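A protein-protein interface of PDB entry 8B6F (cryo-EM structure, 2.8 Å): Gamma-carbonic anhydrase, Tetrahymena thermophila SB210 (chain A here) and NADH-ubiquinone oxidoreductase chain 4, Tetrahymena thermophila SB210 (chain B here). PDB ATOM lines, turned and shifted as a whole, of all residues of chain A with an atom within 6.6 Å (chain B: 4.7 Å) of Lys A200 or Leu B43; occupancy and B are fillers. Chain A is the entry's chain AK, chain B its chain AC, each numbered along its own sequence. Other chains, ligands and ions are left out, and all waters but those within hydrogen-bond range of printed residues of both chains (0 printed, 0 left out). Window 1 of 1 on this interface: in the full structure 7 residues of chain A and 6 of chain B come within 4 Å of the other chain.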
ATOM      1  N   ASN A  92     -21.541   6.191 -30.103  1.00  0.00           N
ATOM      2  CA  ASN A  92     -22.129   5.051 -29.409  1.00  0.00           C
ATOM      3  C   ASN A  92     -23.625   4.945 -29.687  1.00  0.00           C
ATOM      4  O   ASN A  92     -24.423   4.668 -28.791  1.00  0.00           O
ATOM      5  CB  ASN A  92     -21.859   5.141 -27.907  1.00  0.00           C
ATOM      6  CG  ASN A  92     -21.784   3.786 -27.250  1.00  0.00           C
ATOM      7  OD1 ASN A  92     -22.450   2.841 -27.671  1.00  0.00           O
ATOM      8  ND2 ASN A  92     -20.960   3.676 -26.215  1.00  0.00           N
ATOM      9  N   TYR A 120     -25.748   8.013 -27.949  1.00  0.00           N
ATOM     10  CA  TYR A 120     -26.540   6.971 -27.302  1.00  0.00           C
ATOM     11  C   TYR A 120     -27.931   6.831 -27.911  1.00  0.00           C
ATOM     12  O   TYR A 120     -28.850   6.336 -27.252  1.00  0.00           O
ATOM     13  CB  TYR A 120     -26.664   7.228 -25.798  1.00  0.00           C
ATOM     14  CG  TYR A 120     -25.345   7.263 -25.067  1.00  0.00           C
ATOM     15  CD1 TYR A 120     -24.701   6.091 -24.698  1.00  0.00           C
ATOM     16  CD2 TYR A 120     -24.748   8.470 -24.738  1.00  0.00           C
ATOM     17  CE1 TYR A 120     -23.499   6.119 -24.026  1.00  0.00           C
ATOM     18  CE2 TYR A 120     -23.545   8.510 -24.066  1.00  0.00           C
ATOM     19  CZ  TYR A 120     -22.925   7.332 -23.713  1.00  0.00           C
ATOM     20  OH  TYR A 120     -21.725   7.367 -23.044  1.00  0.00           O
ATOM     21  N   ILE A 122     -30.677   5.135 -30.158  1.00  0.00           N
ATOM     22  CA  ILE A 122     -30.986   3.815 -30.692  1.00  0.00           C
ATOM     23  C   ILE A 122     -32.144   3.963 -31.664  1.00  0.00           C
ATOM     24  O   ILE A 122     -33.200   4.496 -31.304  1.00  0.00           O
ATOM     25  CB  ILE A 122     -31.331   2.820 -29.573  1.00  0.00           C
ATOM     26  CG1 ILE A 122     -30.223   2.830 -28.515  1.00  0.00           C
ATOM     27  CG2 ILE A 122     -31.537   1.427 -30.158  1.00  0.00           C
ATOM     28  CD1 ILE A 122     -30.409   1.830 -27.402  1.00  0.00           C
ATOM     29  N   ASN A 195     -32.241   2.633 -21.094  1.00  0.00           N
ATOM     30  CA  ASN A 195     -31.969   2.938 -22.495  1.00  0.00           C
ATOM     31  C   ASN A 195     -30.483   3.176 -22.722  1.00  0.00           C
ATOM     32  O   ASN A 195     -29.898   2.658 -23.679  1.00  0.00           O
ATOM     33  CB  ASN A 195     -32.780   4.156 -22.931  1.00  0.00           C
ATOM     34  CG  ASN A 195     -34.269   3.956 -22.756  1.00  0.00           C
ATOM     35  OD1 ASN A 195     -34.757   2.827 -22.743  1.00  0.00           O
ATOM     36  ND2 ASN A 195     -35.001   5.054 -22.621  1.00  0.00           N
ATOM     37  N   ILE A 196     -29.850   3.951 -21.841  1.00  0.00           N
ATOM     38  CA  ILE A 196     -28.417   4.205 -21.971  1.00  0.00           C
ATOM     39  C   ILE A 196     -27.642   2.899 -21.867  1.00  0.00           C
ATOM     40  O   ILE A 196     -26.665   2.679 -22.590  1.00  0.00           O
ATOM     41  CB  ILE A 196     -27.955   5.221 -20.910  1.00  0.00           C
ATOM     42  CG1 ILE A 196     -28.647   6.566 -21.127  1.00  0.00           C
ATOM     43  CG2 ILE A 196     -26.443   5.398 -20.961  1.00  0.00           C
ATOM     44  CD1 ILE A 196     -28.440   7.552 -19.993  1.00  0.00           C
ATOM     45  N   ASP A 197     -28.071   2.012 -20.969  1.00  0.00           N
ATOM     46  CA  ASP A 197     -27.390   0.734 -20.810  1.00  0.00           C
ATOM     47  C   ASP A 197     -27.494  -0.102 -22.076  1.00  0.00           C
ATOM     48  O   ASP A 197     -26.520  -0.743 -22.489  1.00  0.00           O
ATOM     49  CB  ASP A 197     -27.975  -0.022 -19.620  1.00  0.00           C
ATOM     50  CG  ASP A 197     -27.163  -1.243 -19.252  1.00  0.00           C
ATOM     51  OD1 ASP A 197     -26.131  -1.493 -19.907  1.00  0.00           O
ATOM     52  OD2 ASP A 197     -27.555  -1.952 -18.305  1.00  0.00           O
ATOM     53  N   HIS A 198     -28.668  -0.110 -22.708  1.00  0.00           N
ATOM     54  CA  HIS A 198     -28.820  -0.839 -23.960  1.00  0.00           C
ATOM     55  C   HIS A 198     -27.905  -0.267 -25.036  1.00  0.00           C
ATOM     56  O   HIS A 198     -27.256  -1.017 -25.772  1.00  0.00           O
ATOM     57  CB  HIS A 198     -30.282  -0.798 -24.404  1.00  0.00           C
ATOM     58  CG  HIS A 198     -30.585  -1.688 -25.568  1.00  0.00           C
ATOM     59  ND1 HIS A 198     -31.096  -1.212 -26.757  1.00  0.00           N
ATOM     60  CD2 HIS A 198     -30.454  -3.025 -25.724  1.00  0.00           C
ATOM     61  CE1 HIS A 198     -31.263  -2.218 -27.595  1.00  0.00           C
ATOM     62  NE2 HIS A 198     -30.881  -3.330 -26.994  1.00  0.00           N
ATOM     63  N   ALA A 199     -27.830   1.061 -25.135  1.00  0.00           N
ATOM     64  CA  ALA A 199     -26.949   1.684 -26.118  1.00  0.00           C
ATOM     65  C   ALA A 199     -25.496   1.293 -25.879  1.00  0.00           C
ATOM     66  O   ALA A 199     -24.761   0.991 -26.827  1.00  0.00           O
ATOM     67  CB  ALA A 199     -27.107   3.203 -26.075  1.00  0.00           C
ATOM     68  N   LYS A 200     -25.063   1.296 -24.617  1.00  0.00           N
ATOM     69  CA  LYS A 200     -23.701   0.880 -24.296  1.00  0.00           C
ATOM     70  C   LYS A 200     -23.492  -0.600 -24.567  1.00  0.00           C
ATOM     71  O   LYS A 200     -22.380  -1.015 -24.911  1.00  0.00           O
ATOM     72  CB  LYS A 200     -23.384   1.191 -22.833  1.00  0.00           C
ATOM     73  CG  LYS A 200     -23.333   2.672 -22.508  1.00  0.00           C
ATOM     74  CD  LYS A 200     -23.125   2.904 -21.023  1.00  0.00           C
ATOM     75  CE  LYS A 200     -22.966   4.381 -20.717  1.00  0.00           C
ATOM     76  NZ  LYS A 200     -22.803   4.633 -19.258  1.00  0.00           N
ATOM     77  N   LYS A 201     -24.540  -1.409 -24.417  1.00  0.00           N
ATOM     78  CA  LYS A 201     -24.392  -2.852 -24.554  1.00  0.00           C
ATOM     79  C   LYS A 201     -24.228  -3.275 -26.008  1.00  0.00           C
ATOM     80  O   LYS A 201     -23.564  -4.279 -26.285  1.00  0.00           O
ATOM     81  CB  LYS A 201     -25.602  -3.541 -23.925  1.00  0.00           C
ATOM     82  CG  LYS A 201     -25.518  -5.053 -23.886  1.00  0.00           C
ATOM     83  CD  LYS A 201     -26.707  -5.661 -23.154  1.00  0.00           C
ATOM     84  CE  LYS A 201     -26.713  -5.287 -21.676  1.00  0.00           C
ATOM     85  NZ  LYS A 201     -27.768  -6.016 -20.919  1.00  0.00           N
ATOM     86  N   GLN A 202     -24.821  -2.537 -26.949  1.00  0.00           N
ATOM     87  CA  GLN A 202     -24.680  -2.884 -28.359  1.00  0.00           C
ATOM     88  C   GLN A 202     -23.225  -2.883 -28.813  1.00  0.00           C
ATOM     89  O   GLN A 202     -22.904  -3.511 -29.827  1.00  0.00           O
ATOM     90  CB  GLN A 202     -25.481  -1.911 -29.227  1.00  0.00           C
ATOM     91  CG  GLN A 202     -26.980  -1.937 -28.977  1.00  0.00           C
ATOM     92  CD  GLN A 202     -27.586  -3.309 -29.175  1.00  0.00           C
ATOM     93  OE1 GLN A 202     -28.405  -3.757 -28.372  1.00  0.00           O
ATOM     94  NE2 GLN A 202     -27.195  -3.984 -30.249  1.00  0.00           N
ATOM     95  N   LEU A 203     -22.343  -2.186 -28.094  1.00  0.00           N
ATOM     96  CA  LEU A 203     -20.975  -2.007 -28.569  1.00  0.00           C
ATOM     97  C   LEU A 203     -20.219  -3.328 -28.644  1.00  0.00           C
ATOM     98  O   LEU A 203     -19.500  -3.582 -29.616  1.00  0.00           O
ATOM     99  CB  LEU A 203     -20.234  -1.024 -27.663  1.00  0.00           C
ATOM    100  CG  LEU A 203     -18.740  -0.845 -27.949  1.00  0.00           C
ATOM    101  CD1 LEU A 203     -18.507  -0.398 -29.382  1.00  0.00           C
ATOM    102  CD2 LEU A 203     -18.136   0.149 -26.975  1.00  0.00           C
ATOM    103  N   HIS A 204     -20.366  -4.183 -27.630  1.00  0.00           N
ATOM    104  CA  HIS A 204     -19.594  -5.421 -27.618  1.00  0.00           C
ATOM    105  C   HIS A 204     -20.078  -6.390 -28.687  1.00  0.00           C
ATOM    106  O   HIS A 204     -19.272  -7.137 -29.250  1.00  0.00           O
ATOM    107  CB  HIS A 204     -19.631  -6.076 -26.233  1.00  0.00           C
ATOM    108  CG  HIS A 204     -20.896  -6.816 -25.932  1.00  0.00           C
ATOM    109  ND1 HIS A 204     -21.997  -6.213 -25.361  1.00  0.00           N
ATOM    110  CD2 HIS A 204     -21.228  -8.117 -26.103  1.00  0.00           C
ATOM    111  CE1 HIS A 204     -22.954  -7.110 -25.206  1.00  0.00           C
ATOM    112  NE2 HIS A 204     -22.513  -8.273 -25.646  1.00  0.00           N
ATOM    113  N   GLN B  41     -15.277  -3.310 -19.895  1.00  0.00           N
ATOM    114  CA  GLN B  41     -16.217  -4.391 -19.635  1.00  0.00           C
ATOM    115  C   GLN B  41     -17.088  -4.668 -20.852  1.00  0.00           C
ATOM    116  O   GLN B  41     -17.532  -3.747 -21.541  1.00  0.00           O
ATOM    117  CB  GLN B  41     -17.108  -4.049 -18.444  1.00  0.00           C
ATOM    118  CG  GLN B  41     -17.880  -5.228 -17.892  1.00  0.00           C
ATOM    119  CD  GLN B  41     -18.836  -4.825 -16.796  1.00  0.00           C
ATOM    120  OE1 GLN B  41     -18.832  -3.683 -16.343  1.00  0.00           O
ATOM    121  NE2 GLN B  41     -19.668  -5.764 -16.363  1.00  0.00           N
ATOM    122  N   ASN B  42     -17.325  -5.950 -21.115  1.00  0.00           N
ATOM    123  CA  ASN B  42     -18.351  -6.372 -22.058  1.00  0.00           C
ATOM    124  C   ASN B  42     -19.643  -6.590 -21.283  1.00  0.00           C
ATOM    125  O   ASN B  42     -19.702  -7.444 -20.393  1.00  0.00           O
ATOM    126  CB  ASN B  42     -17.935  -7.649 -22.785  1.00  0.00           C
ATOM    127  CG  ASN B  42     -16.832  -7.413 -23.794  1.00  0.00           C
ATOM    128  OD1 ASN B  42     -16.168  -6.379 -23.774  1.00  0.00           O
ATOM    129  ND2 ASN B  42     -16.633  -8.375 -24.684  1.00  0.00           N
ATOM    130  N   LEU B  43     -20.676  -5.824 -21.620  1.00  0.00           N
ATOM    131  CA  LEU B  43     -21.892  -5.822 -20.816  1.00  0.00           C
ATOM    132  C   LEU B  43     -22.680  -7.107 -21.029  1.00  0.00           C
ATOM    133  O   LEU B  43     -23.764  -7.092 -21.620  1.00  0.00           O
ATOM    134  CB  LEU B  43     -22.744  -4.598 -21.147  1.00  0.00           C
ATOM    135  CG  LEU B  43     -22.031  -3.245 -21.040  1.00  0.00           C
ATOM    136  CD1 LEU B  43     -23.028  -2.108 -21.154  1.00  0.00           C
ATOM    137  CD2 LEU B  43     -21.240  -3.126 -19.748  1.00  0.00           C
ATOM    138  N   ASN B  44     -22.140  -8.220 -20.540  1.00  0.00           N
ATOM    139  CA  ASN B  44     -22.801  -9.511 -20.637  1.00  0.00           C
ATOM    140  C   ASN B  44     -22.337 -10.382 -19.479  1.00  0.00           C
ATOM    141  O   ASN B  44     -21.340 -10.088 -18.815  1.00  0.00           O
ATOM    142  CB  ASN B  44     -22.523 -10.194 -21.981  1.00  0.00           C
ATOM    143  CG  ASN B  44     -21.047 -10.263 -22.308  1.00  0.00           C
ATOM    144  OD1 ASN B  44     -20.200 -10.230 -21.418  1.00  0.00           O
ATOM    145  ND2 ASN B  44     -20.732 -10.356 -23.592  1.00  0.00           N
ATOM    146  N   TYR B 142     -18.049   0.468 -13.330  1.00  0.00           N
ATOM    147  CA  TYR B 142     -18.957   0.051 -14.400  1.00  0.00           C
ATOM    148  C   TYR B 142     -18.389   0.462 -15.759  1.00  0.00           C
ATOM    149  O   TYR B 142     -18.465   1.634 -16.136  1.00  0.00           O
ATOM    150  CB  TYR B 142     -20.344   0.630 -14.189  1.00  0.00           C
ATOM    151  CG  TYR B 142     -21.299   0.302 -15.312  1.00  0.00           C
ATOM    152  CD1 TYR B 142     -21.960  -0.919 -15.358  1.00  0.00           C
ATOM    153  CD2 TYR B 142     -21.533   1.213 -16.332  1.00  0.00           C
ATOM    154  CE1 TYR B 142     -22.831  -1.221 -16.386  1.00  0.00           C
ATOM    155  CE2 TYR B 142     -22.402   0.923 -17.365  1.00  0.00           C
ATOM    156  CZ  TYR B 142     -23.047  -0.296 -17.387  1.00  0.00           C
ATOM    157  OH  TYR B 142     -23.912  -0.586 -18.416  1.00  0.00           O
ATOM    158  N   TRP B 143     -17.830  -0.513 -16.474  1.00  0.00           N
ATOM    159  CA  TRP B 143     -17.692  -0.503 -17.928  1.00  0.00           C
ATOM    160  C   TRP B 143     -16.613   0.417 -18.486  1.00  0.00           C
ATOM    161  O   TRP B 143     -16.263   0.306 -19.664  1.00  0.00           O
ATOM    162  CB  TRP B 143     -19.039  -0.127 -18.558  1.00  0.00           C
ATOM    163  CG  TRP B 143     -18.996   0.027 -20.048  1.00  0.00           C
ATOM    164  CD1 TRP B 143     -18.743  -0.948 -20.967  1.00  0.00           C
ATOM    165  CD2 TRP B 143     -19.220   1.230 -20.793  1.00  0.00           C
ATOM    166  NE1 TRP B 143     -18.793  -0.427 -22.236  1.00  0.00           N
ATOM    167  CE2 TRP B 143     -19.084   0.908 -22.157  1.00  0.00           C
ATOM    168  CE3 TRP B 143     -19.522   2.549 -20.438  1.00  0.00           C
ATOM    169  CZ2 TRP B 143     -19.239   1.856 -23.166  1.00  0.00           C
ATOM    170  CZ3 TRP B 143     -19.673   3.490 -21.442  1.00  0.00           C
ATOM    171  CH2 TRP B 143     -19.532   3.138 -22.792  1.00  0.00           C
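NE2 of His A204 sits close to ND2 of Asn B44.
OH of Tyr B142 lies within hydrogen-bond range of OD1 of Asp A197 (2.8 Å).
OE1 of Gln B41 is in hydrogen-bond range of N of Trp B143 (3.3 Å).
O of Asn B42 lies close to OD1 of Asn B44, 3.0 Å away.
OD1 of Asn A92 sits close to O of Ala A199 (3.1 Å).
O of Lys A201 sits at hydrogen-bond distance from ND1 of His A204, 2.7 Å away.
Among the printed residues, merely in contact across the chains: Asp A197 with Leu B43 (3.4 Å), Lys A201 with Leu B43 (3.5 Å), Lys A200 with Trp B143 (3.5 Å), His A204 with Leu B43 (3.7 Å), Lys A200 with Leu B43 (3.7 Å), Asn A92 with Trp B143 (3.7 Å) and His A204 with Asn B42 (3.9 Å).
Of the printed residues of chain B, Lys A200 touches Leu B43 (3.7 Å) and Trp B143 (3.5 Å).
Leu B43 touches just these residues of chain A: Asp A197, Lys A200, Lys A201 and His A204.
Printed residues of chain B within 4 Å of Asp A197: Leu B43 and Tyr B142.
Of the printed residues of chain A, Asn B42 touches His A204.
Asn A195 touches none of the printed residues of chain B.
The nearest residue of chain A that does not touch Leu B43 is Gln A202 (6.1 Å).
The nearest printed residue of chain B that does not touch His A204 is Gln B41 (5.6 Å).
Hydrophobic or aromatic side chains of chain B within 4 Å of the printed part of chain A: Leu B43, Tyr B142 and Trp B143.
Of the 13 printed residues of chain A, 5 touch a printed residue of chain B.
Printed residues of chain A that touch a printed residue of chain B: Asn A92, Asp A197, Lys A200, Lys A201 and His A204.
Hydrophobic or aromatic side chains of chain A within 4 Å of the printed part of chain B: His A204.
Among the printed residues, 9 pairs touch across the chains.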
